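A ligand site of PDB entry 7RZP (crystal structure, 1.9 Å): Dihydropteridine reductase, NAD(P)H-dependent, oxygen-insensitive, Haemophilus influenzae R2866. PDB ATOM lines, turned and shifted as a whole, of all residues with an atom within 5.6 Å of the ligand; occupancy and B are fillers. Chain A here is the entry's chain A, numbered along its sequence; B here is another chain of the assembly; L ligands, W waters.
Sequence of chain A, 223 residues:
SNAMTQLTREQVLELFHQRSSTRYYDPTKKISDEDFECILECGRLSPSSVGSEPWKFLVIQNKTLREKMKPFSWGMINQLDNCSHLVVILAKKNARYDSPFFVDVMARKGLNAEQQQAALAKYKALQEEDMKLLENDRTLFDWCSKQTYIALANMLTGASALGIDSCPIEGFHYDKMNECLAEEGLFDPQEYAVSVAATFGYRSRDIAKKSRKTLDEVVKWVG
Water W1 lies within hydrogen-bond range of an oxygen (O7) of the ligand (2.8 Å), the side-chain hydroxyl (OG) of Ser 20 (2.9 Å) and the backbone carbonyl oxygen (O) of Ala 208 (3.0 Å).
Water W2 lies within hydrogen-bond range of NH1 of Arg 23 and O7 of the ligand.
Water W3 lies within hydrogen-bond range of N of Ser 211 (3.0 Å), NH1 of Arg 212 (3.0 Å) and O6 of the ligand (3.3 Å).
O7 of the ligand sits at hydrogen-bond distance from N of Ser 21, at 2.9 Å.
The side-chain amino group of Lys 210 is in salt-bridge range of an oxygen (O9) of the ligand.
An oxygen (O8) of the ligand is in salt-bridge range of the guanidinium group (NH1) of Arg 19 (3.0 Å).
NE of Arg 23 sits at hydrogen-bond distance from O1 of the ligand, 2.7 Å away.
The backbone carbonyl oxygen (O) of Gly 75 sits at hydrogen-bond distance from a nitrogen (N2) of the ligand (2.9 Å).
An oxygen (O2) of the ligand sits at hydrogen-bond distance from the backbone NH (N) of Gly 171 (2.9 Å).
The guanidinium group of Arg 212 is in salt-bridge range of an oxygen (O9) of the ligand, 2.8 Å away.
An oxygen (O8) of the ligand is in hydrogen-bond range of the side-chain hydroxyl (OG) of Ser 21 (2.7 Å).
N1 of the ligand is in hydrogen-bond range of SG of Cys 167, 3.7 Å away.
The backbone NH of Gly 51 of chain B lies within hydrogen-bond range of an oxygen (O5) of the ligand (3.4 Å).
The backbone NH of Glu 170 is in hydrogen-bond range of a nitrogen (N3) of the ligand (2.8 Å).
NZ of Lys 109 of chain B lies within hydrogen-bond range of O5 of the ligand (2.9 Å).
NZ of Lys 210 sits at hydrogen-bond distance from O of Arg 19, at 3.0 Å.
OG of Ser 49 of chain B lies within hydrogen-bond range of OE1 of Glu 170, at 2.6 Å.
The side-chain amide nitrogen (NE2) of Gln 147 of chain B sits at hydrogen-bond distance from the side-chain carboxylate (OE2) of Glu 170, 3.0 Å away.
O of Gly 171 lies within hydrogen-bond range of N of Trp 74, 3.3 Å away.
The backbone carbonyl oxygen (O) of Leu 45 of chain B sits at hydrogen-bond distance from the guanidinium group (NH2) of Arg 212 (2.9 Å).
NZ of Lys 210 sits at hydrogen-bond distance from O of Leu 45 of chain B (3.4 Å).
N of Gly 75 lies within hydrogen-bond range of O of Gly 171, 2.7 Å away.
The side-chain carboxylate of Glu 170 is in hydrogen-bond range of the side-chain hydroxyl of Tyr 149, 2.5 Å away.
N4 of the ligand lies close to O of Pro 168.
CA of Ser 20 touches O7 of the ligand (3.7 Å).
Gln 79 touches the ligand.
Tyr 149 touches the ligand.
Ile 169 touches the ligand.
Pro 47 of chain B touches the ligand (CB to O4, 3.4 Å).
Ser 48 of chain B touches the ligand (CA to C9, 3.3 Å).
N of Ser 49 of chain B touches C8 of the ligand, at 3.5 Å.
N of Val 50 of chain B touches O3 of the ligand, 3.9 Å away.
OE1 of Gln 147 of chain B touches C7 of the ligand, at 3.3 Å.
Ile 150 of chain B touches the ligand (CD1 to C9, 3.4 Å).
Hydrophobic or aromatic side chains that line the ligand: Tyr 149, Pro 168, Ile 169, Pro 47 of chain B and Ile 150 of chain B.
22 residues have an atom within 4 Å of the ligand: Arg 19, Ser 20, Ser 21, Arg 23, Gly 75, Gln 79, Tyr 149, Cys 167, Pro 168, Ile 169, Glu 170, Gly 171, Lys 210, Arg 212, Pro 47 of chain B, Ser 48 of chain B, Ser 49 of chain B, Val 50 of chain B, Gly 51 of chain B, Lys 109 of chain B, Gln 147 of chain B and Ile 150 of chain B.
The nearest printed residue that does not touch the ligand is Val 196 (4.1 Å).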
ATOM      1  N   ARG A  19      15.129 -16.395  23.301  1.00  0.00           N
ATOM      2  CA  ARG A  19      14.860 -17.359  24.373  1.00  0.00           C
ATOM      3  C   ARG A  19      14.348 -18.685  23.829  1.00  0.00           C
ATOM      4  O   ARG A  19      13.287 -18.746  23.199  1.00  0.00           O
ATOM      5  CB  ARG A  19      13.904 -16.777  25.406  1.00  0.00           C
ATOM      6  CG  ARG A  19      13.750 -17.717  26.631  1.00  0.00           C
ATOM      7  CD  ARG A  19      12.277 -18.040  26.843  1.00  0.00           C
ATOM      8  NE  ARG A  19      11.619 -18.450  25.602  1.00  0.00           N
ATOM      9  CZ  ARG A  19      11.358 -19.688  25.203  1.00  0.00           C
ATOM     10  NH1 ARG A  19      11.800 -20.746  25.895  1.00  0.00           N
ATOM     11  NH2 ARG A  19      10.641 -19.863  24.091  1.00  0.00           N
ATOM     12  N   SER A  20      15.121 -19.752  24.033  1.00  0.00           N
ATOM     13  CA  SER A  20      14.788 -21.083  23.544  1.00  0.00           C
ATOM     14  C   SER A  20      14.895 -22.055  24.714  1.00  0.00           C
ATOM     15  O   SER A  20      15.418 -21.709  25.784  1.00  0.00           O
ATOM     16  CB  SER A  20      15.703 -21.508  22.395  1.00  0.00           C
ATOM     17  OG  SER A  20      15.114 -21.188  21.149  1.00  0.00           O
ATOM     18  N   SER A  21      14.379 -23.262  24.533  1.00  0.00           N
ATOM     19  CA  SER A  21      14.403 -24.226  25.618  1.00  0.00           C
ATOM     20  C   SER A  21      15.734 -24.967  25.599  1.00  0.00           C
ATOM     21  O   SER A  21      16.065 -25.643  24.625  1.00  0.00           O
ATOM     22  CB  SER A  21      13.192 -25.173  25.517  1.00  0.00           C
ATOM     23  OG  SER A  21      12.039 -24.433  25.898  1.00  0.00           O
ATOM     24  N   ARG A  23      18.160 -27.718  26.738  1.00  0.00           N
ATOM     25  CA  ARG A  23      18.136 -29.052  27.315  1.00  0.00           C
ATOM     26  C   ARG A  23      19.519 -29.621  27.573  1.00  0.00           C
ATOM     27  O   ARG A  23      19.626 -30.679  28.213  1.00  0.00           O
ATOM     28  CB  ARG A  23      17.341 -29.983  26.402  1.00  0.00           C
ATOM     29  CG  ARG A  23      15.976 -29.358  26.169  1.00  0.00           C
ATOM     30  CD  ARG A  23      15.167 -30.131  25.153  1.00  0.00           C
ATOM     31  NE  ARG A  23      13.793 -29.657  25.185  1.00  0.00           N
ATOM     32  CZ  ARG A  23      13.240 -28.884  24.259  1.00  0.00           C
ATOM     33  NH1 ARG A  23      13.931 -28.485  23.193  1.00  0.00           N
ATOM     34  NH2 ARG A  23      11.961 -28.529  24.376  1.00  0.00           N
ATOM     35  N   TRP A  74      11.694 -37.224  33.909  1.00  0.00           N
ATOM     36  CA  TRP A  74      12.211 -37.474  32.569  1.00  0.00           C
ATOM     37  C   TRP A  74      12.368 -36.186  31.753  1.00  0.00           C
ATOM     38  O   TRP A  74      13.217 -36.122  30.856  1.00  0.00           O
ATOM     39  CB  TRP A  74      11.284 -38.438  31.803  1.00  0.00           C
ATOM     40  CG  TRP A  74       9.794 -38.048  31.819  1.00  0.00           C
ATOM     41  CD1 TRP A  74       8.821 -38.499  32.690  1.00  0.00           C
ATOM     42  CD2 TRP A  74       9.132 -37.118  30.951  1.00  0.00           C
ATOM     43  NE1 TRP A  74       7.603 -37.933  32.383  1.00  0.00           N
ATOM     44  CE2 TRP A  74       7.768 -37.071  31.334  1.00  0.00           C
ATOM     45  CE3 TRP A  74       9.563 -36.320  29.873  1.00  0.00           C
ATOM     46  CZ2 TRP A  74       6.841 -36.264  30.678  1.00  0.00           C
ATOM     47  CZ3 TRP A  74       8.625 -35.519  29.224  1.00  0.00           C
ATOM     48  CH2 TRP A  74       7.285 -35.504  29.623  1.00  0.00           C
ATOM     49  N   GLY A  75      11.542 -35.189  32.034  1.00  0.00           N
ATOM     50  CA  GLY A  75      11.611 -33.943  31.288  1.00  0.00           C
ATOM     51  C   GLY A  75      12.904 -33.187  31.465  1.00  0.00           C
ATOM     52  O   GLY A  75      13.219 -32.316  30.642  1.00  0.00           O
ATOM     53  N   MET A  76      13.673 -33.511  32.501  1.00  0.00           N
ATOM     54  CA  MET A  76      14.849 -32.723  32.822  1.00  0.00           C
ATOM     55  C   MET A  76      15.986 -33.584  33.339  1.00  0.00           C
ATOM     56  O   MET A  76      16.893 -33.084  33.999  1.00  0.00           O
ATOM     57  CB  MET A  76      14.515 -31.628  33.839  1.00  0.00           C
ATOM     58  CG  MET A  76      13.757 -32.044  35.110  1.00  0.00           C
ATOM     59  SD  MET A  76      13.973 -30.688  36.557  1.00  0.00           S
ATOM     60  CE  MET A  76      12.710 -31.389  37.841  1.00  0.00           C
ATOM     61  N   GLN A  79      19.355 -32.524  32.318  1.00  0.00           N
ATOM     62  CA  GLN A  79      19.589 -31.149  32.736  1.00  0.00           C
ATOM     63  C   GLN A  79      19.873 -31.039  34.226  1.00  0.00           C
ATOM     64  O   GLN A  79      20.525 -30.081  34.653  1.00  0.00           O
ATOM     65  CB  GLN A  79      18.379 -30.279  32.403  1.00  0.00           C
ATOM     66  CG  GLN A  79      17.822 -30.437  31.010  1.00  0.00           C
ATOM     67  CD  GLN A  79      16.616 -29.541  30.782  1.00  0.00           C
ATOM     68  OE1 GLN A  79      15.702 -29.887  30.017  1.00  0.00           O
ATOM     69  NE2 GLN A  79      16.549 -28.422  31.537  1.00  0.00           N
ATOM     70  N   TYR A 149       2.597 -19.280  36.486  1.00  0.00           N
ATOM     71  CA  TYR A 149       3.191 -19.386  35.164  1.00  0.00           C
ATOM     72  C   TYR A 149       3.538 -18.015  34.616  1.00  0.00           C
ATOM     73  O   TYR A 149       4.391 -17.909  33.711  1.00  0.00           O
ATOM     74  CB  TYR A 149       2.236 -20.111  34.202  1.00  0.00           C
ATOM     75  CG  TYR A 149       2.289 -21.648  34.269  1.00  0.00           C
ATOM     76  CD1 TYR A 149       2.081 -22.328  35.466  1.00  0.00           C
ATOM     77  CD2 TYR A 149       2.554 -22.407  33.125  1.00  0.00           C
ATOM     78  CE1 TYR A 149       2.108 -23.746  35.500  1.00  0.00           C
ATOM     79  CE2 TYR A 149       2.610 -23.816  33.166  1.00  0.00           C
ATOM     80  CZ  TYR A 149       2.387 -24.467  34.345  1.00  0.00           C
ATOM     81  OH  TYR A 149       2.419 -25.848  34.382  1.00  0.00           O
ATOM     82  N   LEU A 152       6.904 -17.732  36.177  1.00  0.00           N
ATOM     83  CA  LEU A 152       7.760 -18.564  35.341  1.00  0.00           C
ATOM     84  C   LEU A 152       8.191 -17.803  34.101  1.00  0.00           C
ATOM     85  O   LEU A 152       9.389 -17.659  33.845  1.00  0.00           O
ATOM     86  CB  LEU A 152       7.047 -19.869  34.984  1.00  0.00           C
ATOM     87  CG  LEU A 152       7.712 -20.649  33.826  1.00  0.00           C
ATOM     88  CD1 LEU A 152       8.981 -21.305  34.307  1.00  0.00           C
ATOM     89  CD2 LEU A 152       6.791 -21.653  33.195  1.00  0.00           C
ATOM     90  N   CYS A 167      15.277 -23.495  30.757  1.00  0.00           N
ATOM     91  CA  CYS A 167      14.270 -24.423  30.235  1.00  0.00           C
ATOM     92  C   CYS A 167      13.133 -24.524  31.241  1.00  0.00           C
ATOM     93  O   CYS A 167      13.381 -24.842  32.412  1.00  0.00           O
ATOM     94  CB  CYS A 167      14.826 -25.818  29.987  1.00  0.00           C
ATOM     95  SG  CYS A 167      13.690 -26.840  28.924  1.00  0.00           S
ATOM     96  N   PRO A 168      11.895 -24.244  30.804  1.00  0.00           N
ATOM     97  CA  PRO A 168      10.724 -24.496  31.658  1.00  0.00           C
ATOM     98  C   PRO A 168      10.422 -25.983  31.645  1.00  0.00           C
ATOM     99  O   PRO A 168      10.641 -26.670  30.642  1.00  0.00           O
ATOM    100  CB  PRO A 168       9.610 -23.705  30.950  1.00  0.00           C
ATOM    101  CG  PRO A 168      10.054 -23.629  29.525  1.00  0.00           C
ATOM    102  CD  PRO A 168      11.538 -23.723  29.480  1.00  0.00           C
ATOM    103  N   ILE A 169       9.903 -26.482  32.764  1.00  0.00           N
ATOM    104  CA  ILE A 169       9.845 -27.929  32.993  1.00  0.00           C
ATOM    105  C   ILE A 169       8.494 -28.321  33.587  1.00  0.00           C
ATOM    106  O   ILE A 169       8.113 -27.830  34.670  1.00  0.00           O
ATOM    107  CB  ILE A 169      10.987 -28.402  33.908  1.00  0.00           C
ATOM    108  CG1 ILE A 169      12.367 -28.081  33.287  1.00  0.00           C
ATOM    109  CG2 ILE A 169      10.849 -29.869  34.206  1.00  0.00           C
ATOM    110  CD1 ILE A 169      12.648 -28.830  31.964  1.00  0.00           C
ATOM    111  N   GLU A 170       7.768 -29.191  32.890  1.00  0.00           N
ATOM    112  CA  GLU A 170       6.617 -29.910  33.406  1.00  0.00           C
ATOM    113  C   GLU A 170       6.824 -31.426  33.477  1.00  0.00           C
ATOM    114  O   GLU A 170       5.981 -32.123  34.072  1.00  0.00           O
ATOM    115  CB  GLU A 170       5.368 -29.642  32.539  1.00  0.00           C
ATOM    116  CG  GLU A 170       4.449 -28.503  33.057  1.00  0.00           C
ATOM    117  CD  GLU A 170       3.320 -28.195  32.069  1.00  0.00           C
ATOM    118  OE1 GLU A 170       3.082 -29.016  31.155  1.00  0.00           O
ATOM    119  OE2 GLU A 170       2.663 -27.136  32.210  1.00  0.00           O
ATOM    120  N   GLY A 171       7.887 -31.953  32.870  1.00  0.00           N
ATOM    121  CA  GLY A 171       7.987 -33.384  32.591  1.00  0.00           C
ATOM    122  C   GLY A 171       8.448 -34.196  33.791  1.00  0.00           C
ATOM    123  O   GLY A 171       9.527 -34.778  33.786  1.00  0.00           O
ATOM    124  N   PHE A 172       7.627 -34.247  34.824  1.00  0.00           N
ATOM    125  CA  PHE A 172       7.926 -35.095  35.970  1.00  0.00           C
ATOM    126  C   PHE A 172       6.601 -35.576  36.547  1.00  0.00           C
ATOM    127  O   PHE A 172       5.545 -34.978  36.308  1.00  0.00           O
ATOM    128  CB  PHE A 172       8.758 -34.343  37.021  1.00  0.00           C
ATOM    129  CG  PHE A 172       8.153 -33.041  37.454  1.00  0.00           C
ATOM    130  CD1 PHE A 172       7.249 -32.985  38.509  1.00  0.00           C
ATOM    131  CD2 PHE A 172       8.447 -31.872  36.762  1.00  0.00           C
ATOM    132  CE1 PHE A 172       6.680 -31.788  38.903  1.00  0.00           C
ATOM    133  CE2 PHE A 172       7.884 -30.662  37.160  1.00  0.00           C
ATOM    134  CZ  PHE A 172       6.991 -30.614  38.226  1.00  0.00           C
ATOM    135  N   VAL A 196       5.203 -25.873  38.632  1.00  0.00           N
ATOM    136  CA  VAL A 196       6.023 -25.960  37.427  1.00  0.00           C
ATOM    137  C   VAL A 196       7.486 -25.766  37.840  1.00  0.00           C
ATOM    138  O   VAL A 196       7.765 -25.339  38.956  1.00  0.00           O
ATOM    139  CB  VAL A 196       5.562 -24.931  36.352  1.00  0.00           C
ATOM    140  CG1 VAL A 196       5.943 -23.506  36.740  1.00  0.00           C
ATOM    141  CG2 VAL A 196       6.149 -25.285  34.970  1.00  0.00           C
ATOM    142  N   ALA A 208      17.575 -24.859  19.107  1.00  0.00           N
ATOM    143  CA  ALA A 208      16.717 -25.243  18.002  1.00  0.00           C
ATOM    144  C   ALA A 208      16.016 -24.035  17.403  1.00  0.00           C
ATOM    145  O   ALA A 208      15.626 -23.104  18.116  1.00  0.00           O
ATOM    146  CB  ALA A 208      15.672 -26.268  18.472  1.00  0.00           C
ATOM    147  N   LYS A 210      13.234 -21.651  16.165  1.00  0.00           N
ATOM    148  CA  LYS A 210      11.891 -21.497  16.679  1.00  0.00           C
ATOM    149  C   LYS A 210      10.946 -22.152  15.680  1.00  0.00           C
ATOM    150  O   LYS A 210      11.190 -22.128  14.477  1.00  0.00           O
ATOM    151  CB  LYS A 210      11.515 -20.014  16.878  1.00  0.00           C
ATOM    152  CG  LYS A 210      11.169 -19.623  18.313  1.00  0.00           C
ATOM    153  CD  LYS A 210      12.393 -19.802  19.198  1.00  0.00           C
ATOM    154  CE  LYS A 210      12.075 -19.709  20.665  1.00  0.00           C
ATOM    155  NZ  LYS A 210      11.188 -18.535  21.117  1.00  0.00           N
ATOM    156  N   SER A 211       9.890 -22.778  16.194  1.00  0.00           N
ATOM    157  CA  SER A 211       8.833 -23.343  15.358  1.00  0.00           C
ATOM    158  C   SER A 211       7.498 -22.972  15.981  1.00  0.00           C
ATOM    159  O   SER A 211       7.166 -23.476  17.056  1.00  0.00           O
ATOM    160  CB  SER A 211       8.973 -24.855  15.243  1.00  0.00           C
ATOM    161  OG  SER A 211       7.824 -25.393  14.613  1.00  0.00           O
ATOM    162  N   ARG A 212       6.717 -22.108  15.328  1.00  0.00           N
ATOM    163  CA  ARG A 212       5.465 -21.643  15.905  1.00  0.00           C
ATOM    164  C   ARG A 212       4.384 -21.630  14.844  1.00  0.00           C
ATOM    165  O   ARG A 212       4.667 -21.617  13.641  1.00  0.00           O
ATOM    166  CB  ARG A 212       5.571 -20.232  16.506  1.00  0.00           C
ATOM    167  CG  ARG A 212       6.421 -20.110  17.750  1.00  0.00           C
ATOM    168  CD  ARG A 212       5.865 -20.882  18.955  1.00  0.00           C
ATOM    169  NE  ARG A 212       6.653 -20.585  20.144  1.00  0.00           N
ATOM    170  CZ  ARG A 212       7.817 -21.149  20.450  1.00  0.00           C
ATOM    171  NH1 ARG A 212       8.354 -22.100  19.692  1.00  0.00           N
ATOM    172  NH2 ARG A 212       8.476 -20.718  21.526  1.00  0.00           N
ATOM    173  N   LEU B  45       5.481 -16.123  20.097  1.00  0.00           N
ATOM    174  CA  LEU B  45       6.787 -16.713  20.304  1.00  0.00           C
ATOM    175  C   LEU B  45       6.954 -17.306  21.699  1.00  0.00           C
ATOM    176  O   LEU B  45       8.022 -17.852  21.992  1.00  0.00           O
ATOM    177  CB  LEU B  45       7.883 -15.664  20.039  1.00  0.00           C
ATOM    178  CG  LEU B  45       7.981 -15.175  18.588  1.00  0.00           C
ATOM    179  CD1 LEU B  45       8.824 -13.918  18.480  1.00  0.00           C
ATOM    180  CD2 LEU B  45       8.560 -16.276  17.715  1.00  0.00           C
ATOM    181  N   PRO B  47       7.039 -19.802  24.845  1.00  0.00           N
ATOM    182  CA  PRO B  47       7.124 -21.247  25.020  1.00  0.00           C
ATOM    183  C   PRO B  47       5.809 -21.771  25.530  1.00  0.00           C
ATOM    184  O   PRO B  47       4.987 -21.026  26.071  1.00  0.00           O
ATOM    185  CB  PRO B  47       8.219 -21.411  26.074  1.00  0.00           C
ATOM    186  CG  PRO B  47       8.051 -20.156  26.954  1.00  0.00           C
ATOM    187  CD  PRO B  47       7.622 -19.073  26.006  1.00  0.00           C
ATOM    188  N   SER B  48       5.632 -23.093  25.431  1.00  0.00           N
ATOM    189  CA  SER B  48       4.456 -23.788  25.935  1.00  0.00           C
ATOM    190  C   SER B  48       4.790 -25.265  26.050  1.00  0.00           C
ATOM    191  O   SER B  48       5.634 -25.786  25.312  1.00  0.00           O
ATOM    192  CB  SER B  48       3.235 -23.567  25.041  1.00  0.00           C
ATOM    193  OG  SER B  48       3.498 -24.038  23.716  1.00  0.00           O
ATOM    194  N   SER B  49       4.113 -25.926  26.984  1.00  0.00           N
ATOM    195  CA  SER B  49       4.392 -27.327  27.242  1.00  0.00           C
ATOM    196  C   SER B  49       4.221 -28.118  25.963  1.00  0.00           C
ATOM    197  O   SER B  49       3.236 -27.937  25.233  1.00  0.00           O
ATOM    198  CB  SER B  49       3.460 -27.845  28.341  1.00  0.00           C
ATOM    199  OG  SER B  49       3.597 -29.250  28.570  1.00  0.00           O
ATOM    200  N   VAL B  50       5.182 -29.018  25.707  1.00  0.00           N
ATOM    201  CA  VAL B  50       5.350 -29.806  24.489  1.00  0.00           C
ATOM    202  C   VAL B  50       5.042 -28.996  23.234  1.00  0.00           C
ATOM    203  O   VAL B  50       4.623 -29.554  22.218  1.00  0.00           O
ATOM    204  CB  VAL B  50       4.526 -31.110  24.527  1.00  0.00           C
ATOM    205  CG1 VAL B  50       4.953 -31.974  25.683  1.00  0.00           C
ATOM    206  CG2 VAL B  50       3.028 -30.850  24.643  1.00  0.00           C
ATOM    207  N   GLY B  51       5.327 -27.689  23.257  1.00  0.00           N
ATOM    208  CA  GLY B  51       5.075 -26.872  22.081  1.00  0.00           C
ATOM    209  C   GLY B  51       3.620 -26.876  21.647  1.00  0.00           C
ATOM    210  O   GLY B  51       3.321 -26.873  20.444  1.00  0.00           O
ATOM    211  N   LYS B 109       6.481 -29.846  14.549  1.00  0.00           N
ATOM    212  CA  LYS B 109       7.797 -30.347  14.912  1.00  0.00           C
ATOM    213  C   LYS B 109       8.398 -31.299  13.876  1.00  0.00           C
ATOM    214  O   LYS B 109       9.448 -31.889  14.126  1.00  0.00           O
ATOM    215  CB  LYS B 109       7.739 -31.011  16.286  1.00  0.00           C
ATOM    216  CG  LYS B 109       7.508 -29.976  17.368  1.00  0.00           C
ATOM    217  CD  LYS B 109       7.479 -30.555  18.760  1.00  0.00           C
ATOM    218  CE  LYS B 109       7.253 -29.446  19.829  1.00  0.00           C
ATOM    219  NZ  LYS B 109       8.428 -28.493  20.002  1.00  0.00           N
ATOM    220  N   LYS B 122       4.803 -40.115  25.031  1.00  0.00           N
ATOM    221  CA  LYS B 122       5.204 -39.086  25.989  1.00  0.00           C
ATOM    222  C   LYS B 122       4.028 -38.188  26.366  1.00  0.00           C
ATOM    223  O   LYS B 122       3.900 -37.778  27.528  1.00  0.00           O
ATOM    224  CB  LYS B 122       6.370 -38.291  25.407  1.00  0.00           C
ATOM    225  CG  LYS B 122       6.788 -37.069  26.196  1.00  0.00           C
ATOM    226  CD  LYS B 122       8.136 -36.500  25.698  1.00  0.00           C
ATOM    227  CE  LYS B 122       8.102 -34.978  25.595  1.00  0.00           C
ATOM    228  NZ  LYS B 122       9.475 -34.318  25.626  1.00  0.00           N
ATOM    229  N   GLN B 147      -0.637 -22.442  30.061  1.00  0.00           N
ATOM    230  CA  GLN B 147       0.270 -22.024  28.984  1.00  0.00           C
ATOM    231  C   GLN B 147      -0.078 -20.629  28.461  1.00  0.00           C
ATOM    232  O   GLN B 147       0.814 -19.825  28.151  1.00  0.00           O
ATOM    233  CB  GLN B 147       0.275 -23.046  27.818  1.00  0.00           C
ATOM    234  CG  GLN B 147       0.292 -24.573  28.169  1.00  0.00           C
ATOM    235  CD  GLN B 147       1.405 -24.954  29.127  1.00  0.00           C
ATOM    236  OE1 GLN B 147       2.583 -24.646  28.875  1.00  0.00           O
ATOM    237  NE2 GLN B 147       1.042 -25.627  30.224  1.00  0.00           N
ATOM    238  N   ILE B 150       1.552 -17.742  30.204  1.00  0.00           N
ATOM    239  CA  ILE B 150       2.893 -17.406  29.712  1.00  0.00           C
ATOM    240  C   ILE B 150       2.785 -16.382  28.589  1.00  0.00           C
ATOM    241  O   ILE B 150       3.474 -15.349  28.595  1.00  0.00           O
ATOM    242  CB  ILE B 150       3.645 -18.682  29.248  1.00  0.00           C
ATOM    243  CG1 ILE B 150       3.772 -19.693  30.381  1.00  0.00           C
ATOM    244  CG2 ILE B 150       5.011 -18.320  28.590  1.00  0.00           C
ATOM    245  CD1 ILE B 150       4.545 -20.991  29.991  1.00  0.00           C
HETATM  246  N1  LIG L   1      10.987 -29.044  27.624  1.00  0.00           N
HETATM  247  C1  LIG L   1      11.703 -30.089  28.141  1.00  0.00           C
HETATM  248  O1  LIG L   1      12.789 -30.409  27.593  1.00  0.00           O
HETATM  249  N2  LIG L   1      11.274 -30.776  29.225  1.00  0.00           N
HETATM  250  C2  LIG L   1      10.209 -30.379  29.954  1.00  0.00           C
HETATM  251  O2  LIG L   1       9.832 -31.025  30.950  1.00  0.00           O
HETATM  252  C3  LIG L   1       9.398 -29.240  29.472  1.00  0.00           C
HETATM  253  N3  LIG L   1       8.337 -28.752  30.156  1.00  0.00           N
HETATM  254  C4  LIG L   1       7.767 -27.558  29.837  1.00  0.00           C
HETATM  255  C5  LIG L   1       6.737 -27.031  30.621  1.00  0.00           C
HETATM  256  C6  LIG L   1       6.155 -25.831  30.246  1.00  0.00           C
HETATM  257  C7  LIG L   1       5.055 -25.197  31.058  1.00  0.00           C
HETATM  258  C8  LIG L   1       6.725 -25.069  29.111  1.00  0.00           C
HETATM  259  C9  LIG L   1       6.139 -23.739  28.772  1.00  0.00           C
HETATM  260  C10 LIG L   1       7.700 -25.600  28.294  1.00  0.00           C
HETATM  261  C11 LIG L   1       8.207 -26.857  28.599  1.00  0.00           C
HETATM  262  N4  LIG L   1       9.322 -27.331  27.884  1.00  0.00           N
HETATM  263  C12 LIG L   1       9.964 -28.506  28.328  1.00  0.00           C
HETATM  264  C13 LIG L   1       9.848 -26.638  26.693  1.00  0.00           C
HETATM  265  C14 LIG L   1       8.910 -26.795  25.469  1.00  0.00           C
HETATM  266  O3  LIG L   1       8.858 -28.138  24.967  1.00  0.00           O
HETATM  267  C15 LIG L   1       9.360 -25.797  24.396  1.00  0.00           C
HETATM  268  O4  LIG L   1       9.076 -24.497  24.914  1.00  0.00           O
HETATM  269  C16 LIG L   1       8.782 -25.963  22.981  1.00  0.00           C
HETATM  270  O5  LIG L   1       8.610 -27.338  22.631  1.00  0.00           O
HETATM  271  C17 LIG L   1       9.834 -25.518  21.994  1.00  0.00           C
HETATM  272  O6  LIG L   1       9.969 -24.126  22.031  1.00  0.00           O
HETATM  273  P1  LIG L   1      11.207 -23.228  22.547  1.00  0.00           P
HETATM  274  O7  LIG L   1      12.567 -23.870  22.386  1.00  0.00           O
HETATM  275  O8  LIG L   1      10.943 -22.880  24.026  1.00  0.00           O
HETATM  276  O9  LIG L   1      10.858 -22.130  21.580  1.00  0.00           O
HETATM  277  O   HOH W   1      13.146 -22.901  19.828  1.00  0.00           O
HETATM  278  O   HOH W   2      12.310 -26.958  21.579  1.00  0.00           O
HETATM  279  O   HOH W   3      10.496 -24.033  18.812  1.00  0.00           O
